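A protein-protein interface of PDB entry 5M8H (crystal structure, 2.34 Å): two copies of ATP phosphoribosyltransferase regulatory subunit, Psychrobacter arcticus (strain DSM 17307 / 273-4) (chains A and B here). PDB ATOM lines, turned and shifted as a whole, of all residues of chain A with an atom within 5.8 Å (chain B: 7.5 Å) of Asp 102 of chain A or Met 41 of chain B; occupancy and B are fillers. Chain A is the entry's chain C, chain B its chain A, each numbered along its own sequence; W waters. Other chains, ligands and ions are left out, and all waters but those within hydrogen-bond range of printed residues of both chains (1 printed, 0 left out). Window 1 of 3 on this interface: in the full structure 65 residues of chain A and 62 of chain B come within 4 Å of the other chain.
Water W1 lies within hydrogen-bond range of OD2 of Asp 102 of chain A (3.1 Å) and O of Pro 39 of chain B (3.1 Å).
Met 41 of chain A touches its own counterpart, Met 41 of chain B.
Met 41 of chain A touches Asp 102 of chain B, and with the chains exchanged Asp 102 of chain A touches Met 41 of chain B.
Met 41 of chain A touches Ile 104 of chain B, and with the chains exchanged Ile 104 of chain A touches Met 41 of chain B.
Of the 7 pairs that touch across the chains among the printed residues, 5 have their exchanged pair printed and touching as well.
The backbone carbonyl oxygen (O) of Arg 75 of chain A lies within hydrogen-bond range of the backbone NH (N) of Ile 104 of chain A (2.9 Å).
The backbone carbonyl oxygen of Met 41 of chain A is in hydrogen-bond range of the backbone NH of Arg 75 of chain A (2.9 Å).
The backbone NH (N) of Arg 75 of chain B is in hydrogen-bond range of the backbone carbonyl oxygen (O) of Met 41 of chain B, 2.9 Å away.
The guanidinium group of Arg 75 of chain B sits at hydrogen-bond distance from the backbone carbonyl oxygen of Asp 102 of chain B (2.9 Å).
The backbone NH of Ile 104 of chain B lies within hydrogen-bond range of the backbone carbonyl oxygen of Arg 75 of chain B, 2.9 Å away.
The backbone carbonyl oxygen (O) of Asp 102 of chain A sits at hydrogen-bond distance from the guanidinium group (NE) of Arg 75 of chain A.
Printed residues of chain A that touch a printed residue of chain B: Met 41, Asp 102, Ile 104 and Thr 116.
Hydrophobic or aromatic side chains of chain A within 4 Å of the printed part of chain B: Met 41 and Ile 104.
Among the printed residues, 7 pairs touch across the chains.
Among the printed residues, no Asp or Glu carboxylate lies within 4 Å of a Lys or Arg side-chain nitrogen of the other chain.
Of chain B, only Met 41 comes within 4 Å of Asp 102 of chain A.
Of the printed residues of chain A, Asp 102 of chain B touches Met 41 (3.8 Å).
Printed residues of chain B within 4 Å of Thr 116 of chain A: Ile 42 (3.98 Å).
Pro 39 of chain B touches none of the printed residues of chain A.
The nearest residue of chain A that does not touch Met 41 of chain B is Thr 116 of chain A (5.1 Å).
The nearest printed residue of chain B that does not touch Met 41 of chain A is Ile 74 of chain B (5.7 Å).
Among the printed residues, merely in contact across the chains: Met 41 of chain A with Met 41 of chain B (3.5 Å), Met 41 of chain A with Asp 102 of chain B (3.8 Å), Met 41 of chain A with Ile 104 of chain B (3.6 Å), Asp 102 of chain A with Met 41 of chain B (3.8 Å), Ile 104 of chain A with Met 41 of chain B (3.8 Å), Ile 104 of chain A with Ile 42 of chain B (3.9 Å) and Thr 116 of chain A with Ile 42 of chain B (3.98 Å).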
ATOM      1  N   MET A  41     -35.861  -2.413   4.040  1.00  0.00           N
ATOM      2  CA  MET A  41     -34.945  -3.349   4.690  1.00  0.00           C
ATOM      3  C   MET A  41     -35.455  -3.882   6.019  1.00  0.00           C
ATOM      4  O   MET A  41     -34.988  -4.912   6.464  1.00  0.00           O
ATOM      5  CB  MET A  41     -33.617  -2.677   4.986  1.00  0.00           C
ATOM      6  CG  MET A  41     -32.829  -2.228   3.759  1.00  0.00           C
ATOM      7  SD  MET A  41     -31.983  -3.565   2.977  1.00  0.00           S
ATOM      8  CE  MET A  41     -30.687  -3.726   4.203  1.00  0.00           C
ATOM      9  N   ARG A  75     -34.499  -7.729   6.996  1.00  0.00           N
ATOM     10  CA  ARG A  75     -34.838  -8.842   6.127  1.00  0.00           C
ATOM     11  C   ARG A  75     -33.632  -9.706   5.769  1.00  0.00           C
ATOM     12  O   ARG A  75     -32.562  -9.212   5.454  1.00  0.00           O
ATOM     13  CB  ARG A  75     -35.494  -8.359   4.837  1.00  0.00           C
ATOM     14  CG  ARG A  75     -34.615  -7.485   3.953  1.00  0.00           C
ATOM     15  CD  ARG A  75     -35.427  -6.930   2.804  1.00  0.00           C
ATOM     16  NE  ARG A  75     -34.585  -6.177   1.876  1.00  0.00           N
ATOM     17  CZ  ARG A  75     -35.042  -5.372   0.930  1.00  0.00           C
ATOM     18  NH1 ARG A  75     -36.348  -5.183   0.742  1.00  0.00           N
ATOM     19  NH2 ARG A  75     -34.178  -4.748   0.161  1.00  0.00           N
ATOM     20  N   ILE A  78     -36.451 -11.550   0.692  1.00  0.00           N
ATOM     21  CA  ILE A  78     -37.420 -10.580   0.170  1.00  0.00           C
ATOM     22  C   ILE A  78     -38.761 -11.236  -0.115  1.00  0.00           C
ATOM     23  O   ILE A  78     -39.800 -10.559  -0.046  1.00  0.00           O
ATOM     24  CB  ILE A  78     -36.850  -9.842  -1.069  1.00  0.00           C
ATOM     25  CG1 ILE A  78     -35.738  -8.902  -0.606  1.00  0.00           C
ATOM     26  CG2 ILE A  78     -37.903  -9.009  -1.797  1.00  0.00           C
ATOM     27  CD1 ILE A  78     -34.823  -8.431  -1.712  1.00  0.00           C
ATOM     28  N   ALA A 100     -34.803  -6.261  -6.435  1.00  0.00           N
ATOM     29  CA  ALA A 100     -33.375  -6.341  -6.238  1.00  0.00           C
ATOM     30  C   ALA A 100     -33.031  -5.487  -5.051  1.00  0.00           C
ATOM     31  O   ALA A 100     -33.305  -4.290  -5.030  1.00  0.00           O
ATOM     32  CB  ALA A 100     -32.636  -5.852  -7.459  1.00  0.00           C
ATOM     33  N   GLY A 101     -32.508  -6.117  -4.010  1.00  0.00           N
ATOM     34  CA  GLY A 101     -32.208  -5.392  -2.791  1.00  0.00           C
ATOM     35  C   GLY A 101     -31.320  -6.184  -1.868  1.00  0.00           C
ATOM     36  O   GLY A 101     -31.218  -7.404  -1.968  1.00  0.00           O
ATOM     37  N   ASP A 102     -30.671  -5.462  -0.973  1.00  0.00           N
ATOM     38  CA  ASP A 102     -29.814  -6.031   0.038  1.00  0.00           C
ATOM     39  C   ASP A 102     -30.637  -6.802   1.074  1.00  0.00           C
ATOM     40  O   ASP A 102     -31.686  -6.350   1.493  1.00  0.00           O
ATOM     41  CB  ASP A 102     -29.015  -4.918   0.734  1.00  0.00           C
ATOM     42  CG  ASP A 102     -27.962  -4.264  -0.159  1.00  0.00           C
ATOM     43  OD1 ASP A 102     -27.316  -4.951  -0.959  1.00  0.00           O
ATOM     44  OD2 ASP A 102     -27.726  -3.055  -0.030  1.00  0.00           O
ATOM     45  N   VAL A 103     -30.157  -7.979   1.434  1.00  0.00           N
ATOM     46  CA  VAL A 103     -30.662  -8.734   2.553  1.00  0.00           C
ATOM     47  C   VAL A 103     -29.458  -9.088   3.435  1.00  0.00           C
ATOM     48  O   VAL A 103     -28.337  -9.108   2.967  1.00  0.00           O
ATOM     49  CB  VAL A 103     -31.421 -10.012   2.125  1.00  0.00           C
ATOM     50  CG1 VAL A 103     -32.594  -9.681   1.236  1.00  0.00           C
ATOM     51  CG2 VAL A 103     -30.531 -10.993   1.403  1.00  0.00           C
ATOM     52  N   ILE A 104     -29.712  -9.344   4.713  1.00  0.00           N
ATOM     53  CA  ILE A 104     -28.654  -9.620   5.676  1.00  0.00           C
ATOM     54  C   ILE A 104     -28.958 -10.937   6.372  1.00  0.00           C
ATOM     55  O   ILE A 104     -30.104 -11.202   6.716  1.00  0.00           O
ATOM     56  CB  ILE A 104     -28.553  -8.543   6.764  1.00  0.00           C
ATOM     57  CG1 ILE A 104     -28.598  -7.127   6.180  1.00  0.00           C
ATOM     58  CG2 ILE A 104     -27.295  -8.752   7.587  1.00  0.00           C
ATOM     59  CD1 ILE A 104     -27.391  -6.720   5.401  1.00  0.00           C
ATOM     60  N   THR A 116     -24.202 -10.686   3.279  1.00  0.00           N
ATOM     61  CA  THR A 116     -24.818  -9.479   2.737  1.00  0.00           C
ATOM     62  C   THR A 116     -25.044  -9.562   1.238  1.00  0.00           C
ATOM     63  O   THR A 116     -24.516  -8.750   0.479  1.00  0.00           O
ATOM     64  CB  THR A 116     -23.952  -8.245   2.994  1.00  0.00           C
ATOM     65  OG1 THR A 116     -22.678  -8.415   2.360  1.00  0.00           O
ATOM     66  CG2 THR A 116     -23.794  -8.014   4.471  1.00  0.00           C
ATOM     67  N   PRO A 117     -25.859 -10.517   0.803  1.00  0.00           N
ATOM     68  CA  PRO A 117     -26.075 -10.653  -0.620  1.00  0.00           C
ATOM     69  C   PRO A 117     -26.972  -9.552  -1.170  1.00  0.00           C
ATOM     70  O   PRO A 117     -27.773  -8.989  -0.427  1.00  0.00           O
ATOM     71  CB  PRO A 117     -26.753 -12.027  -0.731  1.00  0.00           C
ATOM     72  CG  PRO A 117     -27.455 -12.197   0.551  1.00  0.00           C
ATOM     73  CD  PRO A 117     -26.577 -11.549   1.570  1.00  0.00           C
ATOM     74  N   LEU A 118     -26.796  -9.238  -2.454  1.00  0.00           N
ATOM     75  CA  LEU A 118     -27.685  -8.324  -3.172  1.00  0.00           C
ATOM     76  C   LEU A 118     -28.684  -9.209  -3.899  1.00  0.00           C
ATOM     77  O   LEU A 118     -28.399  -9.744  -4.974  1.00  0.00           O
ATOM     78  CB  LEU A 118     -26.885  -7.466  -4.137  1.00  0.00           C
ATOM     79  CG  LEU A 118     -27.577  -6.596  -5.177  1.00  0.00           C
ATOM     80  CD1 LEU A 118     -28.742  -5.834  -4.588  1.00  0.00           C
ATOM     81  CD2 LEU A 118     -26.552  -5.628  -5.767  1.00  0.00           C
ATOM     82  N   GLN A 119     -29.837  -9.416  -3.270  1.00  0.00           N
ATOM     83  CA  GLN A 119     -30.783 -10.450  -3.699  1.00  0.00           C
ATOM     84  C   GLN A 119     -31.668  -9.915  -4.821  1.00  0.00           C
ATOM     85  O   GLN A 119     -32.448  -8.966  -4.613  1.00  0.00           O
ATOM     86  CB  GLN A 119     -31.664 -10.930  -2.524  1.00  0.00           C
ATOM     87  CG  GLN A 119     -32.773 -11.937  -2.925  1.00  0.00           C
ATOM     88  CD  GLN A 119     -33.580 -12.485  -1.749  1.00  0.00           C
ATOM     89  OE1 GLN A 119     -34.357 -11.796  -1.115  1.00  0.00           O
ATOM     90  NE2 GLN A 119     -33.411 -13.739  -1.489  1.00  0.00           N
ATOM     91  N   ARG B  22     -31.761   6.485  -9.487  1.00  0.00           N
ATOM     92  CA  ARG B  22     -30.552   6.019  -8.842  1.00  0.00           C
ATOM     93  C   ARG B  22     -29.468   5.733  -9.891  1.00  0.00           C
ATOM     94  O   ARG B  22     -28.315   6.118  -9.723  1.00  0.00           O
ATOM     95  CB  ARG B  22     -30.837   4.748  -8.049  1.00  0.00           C
ATOM     96  CG  ARG B  22     -29.714   4.200  -7.195  1.00  0.00           C
ATOM     97  CD  ARG B  22     -29.661   2.709  -7.358  1.00  0.00           C
ATOM     98  NE  ARG B  22     -28.638   2.154  -6.489  1.00  0.00           N
ATOM     99  CZ  ARG B  22     -28.840   1.241  -5.545  1.00  0.00           C
ATOM    100  NH1 ARG B  22     -30.069   0.739  -5.325  1.00  0.00           N
ATOM    101  NH2 ARG B  22     -27.796   0.820  -4.804  1.00  0.00           N
ATOM    102  N   SER B  38     -19.323   0.638  -3.162  1.00  0.00           N
ATOM    103  CA  SER B  38     -20.526   0.067  -2.605  1.00  0.00           C
ATOM    104  C   SER B  38     -20.121  -0.685  -1.344  1.00  0.00           C
ATOM    105  O   SER B  38     -19.932  -1.896  -1.364  1.00  0.00           O
ATOM    106  CB  SER B  38     -21.253  -0.804  -3.617  1.00  0.00           C
ATOM    107  OG  SER B  38     -22.460  -1.274  -3.074  1.00  0.00           O
ATOM    108  N   PRO B  39     -19.956   0.056  -0.230  1.00  0.00           N
ATOM    109  CA  PRO B  39     -19.690  -0.621   1.037  1.00  0.00           C
ATOM    110  C   PRO B  39     -20.918  -1.373   1.554  1.00  0.00           C
ATOM    111  O   PRO B  39     -22.041  -1.108   1.103  1.00  0.00           O
ATOM    112  CB  PRO B  39     -19.308   0.516   1.990  1.00  0.00           C
ATOM    113  CG  PRO B  39     -19.632   1.804   1.284  1.00  0.00           C
ATOM    114  CD  PRO B  39     -20.164   1.510  -0.075  1.00  0.00           C
ATOM    115  N   PRO B  40     -20.713  -2.309   2.485  1.00  0.00           N
ATOM    116  CA  PRO B  40     -21.822  -3.129   2.960  1.00  0.00           C
ATOM    117  C   PRO B  40     -22.748  -2.383   3.936  1.00  0.00           C
ATOM    118  O   PRO B  40     -22.385  -1.328   4.449  1.00  0.00           O
ATOM    119  CB  PRO B  40     -21.116  -4.288   3.666  1.00  0.00           C
ATOM    120  CG  PRO B  40     -19.848  -3.679   4.168  1.00  0.00           C
ATOM    121  CD  PRO B  40     -19.512  -2.488   3.310  1.00  0.00           C
ATOM    122  N   MET B  41     -23.923  -2.954   4.171  1.00  0.00           N
ATOM    123  CA  MET B  41     -24.895  -2.397   5.106  1.00  0.00           C
ATOM    124  C   MET B  41     -24.477  -2.499   6.569  1.00  0.00           C
ATOM    125  O   MET B  41     -24.994  -1.757   7.377  1.00  0.00           O
ATOM    126  CB  MET B  41     -26.208  -3.168   5.012  1.00  0.00           C
ATOM    127  CG  MET B  41     -26.973  -3.022   3.725  1.00  0.00           C
ATOM    128  SD  MET B  41     -27.711  -1.415   3.414  1.00  0.00           S
ATOM    129  CE  MET B  41     -28.565  -0.998   4.920  1.00  0.00           C
ATOM    130  N   ILE B  42     -23.603  -3.452   6.904  1.00  0.00           N
ATOM    131  CA  ILE B  42     -23.183  -3.704   8.279  1.00  0.00           C
ATOM    132  C   ILE B  42     -21.670  -3.771   8.392  1.00  0.00           C
ATOM    133  O   ILE B  42     -20.990  -4.221   7.477  1.00  0.00           O
ATOM    134  CB  ILE B  42     -23.796  -4.985   8.861  1.00  0.00           C
ATOM    135  CG1 ILE B  42     -23.474  -6.198   8.003  1.00  0.00           C
ATOM    136  CG2 ILE B  42     -25.309  -4.825   8.962  1.00  0.00           C
ATOM    137  CD1 ILE B  42     -23.769  -7.524   8.694  1.00  0.00           C
ATOM    138  N   GLU B  43     -21.167  -3.274   9.522  1.00  0.00           N
ATOM    139  CA  GLU B  43     -19.765  -3.360   9.907  1.00  0.00           C
ATOM    140  C   GLU B  43     -19.712  -3.541  11.416  1.00  0.00           C
ATOM    141  O   GLU B  43     -20.711  -3.332  12.096  1.00  0.00           O
ATOM    142  CB  GLU B  43     -19.051  -2.057   9.604  1.00  0.00           C
ATOM    143  CG  GLU B  43     -19.002  -1.638   8.165  1.00  0.00           C
ATOM    144  CD  GLU B  43     -18.098  -0.465   7.888  1.00  0.00           C
ATOM    145  OE1 GLU B  43     -17.305  -0.040   8.779  1.00  0.00           O
ATOM    146  OE2 GLU B  43     -18.170  -0.010   6.723  1.00  0.00           O
ATOM    147  N   LEU B  48     -17.464   1.426  11.955  1.00  0.00           N
ATOM    148  CA  LEU B  48     -18.639   2.159  11.505  1.00  0.00           C
ATOM    149  C   LEU B  48     -18.873   3.436  12.260  1.00  0.00           C
ATOM    150  O   LEU B  48     -19.291   4.434  11.676  1.00  0.00           O
ATOM    151  CB  LEU B  48     -19.891   1.297  11.646  1.00  0.00           C
ATOM    152  CG  LEU B  48     -21.173   1.838  11.028  1.00  0.00           C
ATOM    153  CD1 LEU B  48     -21.020   2.028   9.540  1.00  0.00           C
ATOM    154  CD2 LEU B  48     -22.305   0.880  11.335  1.00  0.00           C
ATOM    155  N   ILE B  63     -26.504  -4.692  16.352  1.00  0.00           N
ATOM    156  CA  ILE B  63     -26.787  -6.119  16.246  1.00  0.00           C
ATOM    157  C   ILE B  63     -25.517  -6.867  16.646  1.00  0.00           C
ATOM    158  O   ILE B  63     -24.426  -6.277  16.693  1.00  0.00           O
ATOM    159  CB  ILE B  63     -27.232  -6.524  14.829  1.00  0.00           C
ATOM    160  CG1 ILE B  63     -26.258  -5.979  13.758  1.00  0.00           C
ATOM    161  CG2 ILE B  63     -28.641  -6.013  14.539  1.00  0.00           C
ATOM    162  CD1 ILE B  63     -26.517  -6.442  12.342  1.00  0.00           C
ATOM    163  N   GLY B  73     -23.038  -2.620  13.672  1.00  0.00           N
ATOM    164  CA  GLY B  73     -24.130  -1.674  13.372  1.00  0.00           C
ATOM    165  C   GLY B  73     -24.676  -1.824  11.950  1.00  0.00           C
ATOM    166  O   GLY B  73     -23.985  -2.317  11.077  1.00  0.00           O
ATOM    167  N   ILE B  74     -25.929  -1.437  11.750  1.00  0.00           N
ATOM    168  CA  ILE B  74     -26.467  -1.212  10.422  1.00  0.00           C
ATOM    169  C   ILE B  74     -26.205   0.255  10.148  1.00  0.00           C
ATOM    170  O   ILE B  74     -26.577   1.099  10.942  1.00  0.00           O
ATOM    171  CB  ILE B  74     -27.983  -1.433  10.312  1.00  0.00           C
ATOM    172  CG1 ILE B  74     -28.418  -2.755  10.910  1.00  0.00           C
ATOM    173  CG2 ILE B  74     -28.410  -1.451   8.859  1.00  0.00           C
ATOM    174  CD1 ILE B  74     -29.901  -2.753  11.221  1.00  0.00           C
ATOM    175  N   ARG B  75     -25.579   0.570   9.029  1.00  0.00           N
ATOM    176  CA  ARG B  75     -25.206   1.941   8.756  1.00  0.00           C
ATOM    177  C   ARG B  75     -26.400   2.878   8.719  1.00  0.00           C
ATOM    178  O   ARG B  75     -27.435   2.574   8.143  1.00  0.00           O
ATOM    179  CB  ARG B  75     -24.442   2.049   7.438  1.00  0.00           C
ATOM    180  CG  ARG B  75     -25.247   1.649   6.196  1.00  0.00           C
ATOM    181  CD  ARG B  75     -24.375   1.652   4.981  1.00  0.00           C
ATOM    182  NE  ARG B  75     -25.134   1.389   3.767  1.00  0.00           N
ATOM    183  CZ  ARG B  75     -24.596   1.078   2.591  1.00  0.00           C
ATOM    184  NH1 ARG B  75     -23.272   0.982   2.435  1.00  0.00           N
ATOM    185  NH2 ARG B  75     -25.396   0.870   1.554  1.00  0.00           N
ATOM    186  N   ALA B  76     -26.239   4.005   9.385  1.00  0.00           N
ATOM    187  CA  ALA B  76     -27.152   5.121   9.298  1.00  0.00           C
ATOM    188  C   ALA B  76     -26.612   6.189   8.358  1.00  0.00           C
ATOM    189  O   ALA B  76     -27.351   7.072   7.952  1.00  0.00           O
ATOM    190  CB  ALA B  76     -27.357   5.699  10.689  1.00  0.00           C
ATOM    191  N   ILE B  78     -23.308   6.722   5.135  1.00  0.00           N
ATOM    192  CA  ILE B  78     -22.291   6.060   4.308  1.00  0.00           C
ATOM    193  C   ILE B  78     -20.928   6.743   4.421  1.00  0.00           C
ATOM    194  O   ILE B  78     -19.883   6.094   4.258  1.00  0.00           O
ATOM    195  CB  ILE B  78     -22.766   5.935   2.841  1.00  0.00           C
ATOM    196  CG1 ILE B  78     -23.897   4.907   2.783  1.00  0.00           C
ATOM    197  CG2 ILE B  78     -21.663   5.479   1.894  1.00  0.00           C
ATOM    198  CD1 ILE B  78     -24.744   4.963   1.522  1.00  0.00           C
ATOM    199  N   GLN B  81     -17.950   5.209   6.047  1.00  0.00           N
ATOM    200  CA  GLN B  81     -17.443   4.084   5.282  1.00  0.00           C
ATOM    201  C   GLN B  81     -16.540   4.560   4.146  1.00  0.00           C
ATOM    202  O   GLN B  81     -15.549   3.906   3.831  1.00  0.00           O
ATOM    203  CB  GLN B  81     -18.574   3.265   4.721  1.00  0.00           C
ATOM    204  CG  GLN B  81     -19.554   2.743   5.736  1.00  0.00           C
ATOM    205  CD  GLN B  81     -20.603   1.897   5.064  1.00  0.00           C
ATOM    206  OE1 GLN B  81     -21.367   2.391   4.240  1.00  0.00           O
ATOM    207  NE2 GLN B  81     -20.626   0.619   5.378  1.00  0.00           N
ATOM    208  N   ALA B 100     -24.386   5.033  -3.642  1.00  0.00           N
ATOM    209  CA  ALA B 100     -25.825   5.033  -3.515  1.00  0.00           C
ATOM    210  C   ALA B 100     -26.205   3.746  -2.824  1.00  0.00           C
ATOM    211  O   ALA B 100     -25.893   2.667  -3.289  1.00  0.00           O
ATOM    212  CB  ALA B 100     -26.507   5.161  -4.861  1.00  0.00           C
ATOM    213  N   GLY B 101     -26.860   3.864  -1.687  1.00  0.00           N
ATOM    214  CA  GLY B 101     -27.245   2.696  -0.928  1.00  0.00           C
ATOM    215  C   GLY B 101     -28.201   3.013   0.186  1.00  0.00           C
ATOM    216  O   GLY B 101     -28.315   4.160   0.617  1.00  0.00           O
ATOM    217  N   ASP B 102     -28.892   1.969   0.643  1.00  0.00           N
ATOM    218  CA  ASP B 102     -29.807   2.073   1.755  1.00  0.00           C
ATOM    219  C   ASP B 102     -29.047   2.322   3.061  1.00  0.00           C
ATOM    220  O   ASP B 102     -28.002   1.734   3.306  1.00  0.00           O
ATOM    221  CB  ASP B 102     -30.632   0.793   1.900  1.00  0.00           C
ATOM    222  CG  ASP B 102     -31.663   0.605   0.788  1.00  0.00           C
ATOM    223  OD1 ASP B 102     -32.217   1.549   0.216  1.00  0.00           O
ATOM    224  OD2 ASP B 102     -31.959  -0.552   0.507  1.00  0.00           O
ATOM    225  N   VAL B 103     -29.581   3.240   3.858  1.00  0.00           N
ATOM    226  CA  VAL B 103     -29.164   3.427   5.226  1.00  0.00           C
ATOM    227  C   VAL B 103     -30.421   3.344   6.093  1.00  0.00           C
ATOM    228  O   VAL B 103     -31.524   3.567   5.608  1.00  0.00           O
ATOM    229  CB  VAL B 103     -28.418   4.754   5.440  1.00  0.00           C
ATOM    230  CG1 VAL B 103     -27.167   4.823   4.578  1.00  0.00           C
ATOM    231  CG2 VAL B 103     -29.300   5.952   5.161  1.00  0.00           C
ATOM    232  N   ILE B 104     -30.244   3.000   7.360  1.00  0.00           N
ATOM    233  CA  ILE B 104     -31.359   2.829   8.283  1.00  0.00           C
ATOM    234  C   ILE B 104     -31.137   3.706   9.500  1.00  0.00           C
ATOM    235  O   ILE B 104     -30.016   3.799  10.000  1.00  0.00           O
ATOM    236  CB  ILE B 104     -31.481   1.386   8.782  1.00  0.00           C
ATOM    237  CG1 ILE B 104     -31.409   0.376   7.625  1.00  0.00           C
ATOM    238  CG2 ILE B 104     -32.786   1.205   9.537  1.00  0.00           C
ATOM    239  CD1 ILE B 104     -32.585   0.376   6.678  1.00  0.00           C
ATOM    240  N   PRO B 117     -33.924   5.782   4.132  1.00  0.00           N
ATOM    241  CA  PRO B 117     -33.625   6.543   2.918  1.00  0.00           C
ATOM    242  C   PRO B 117     -32.667   5.783   2.003  1.00  0.00           C
ATOM    243  O   PRO B 117     -31.894   4.939   2.476  1.00  0.00           O
ATOM    244  CB  PRO B 117     -32.966   7.808   3.456  1.00  0.00           C
ATOM    245  CG  PRO B 117     -32.358   7.391   4.728  1.00  0.00           C
ATOM    246  CD  PRO B 117     -33.275   6.361   5.320  1.00  0.00           C
HETATM  247  O   HOH W   1     -24.738  -2.253   0.059  1.00  0.00           O
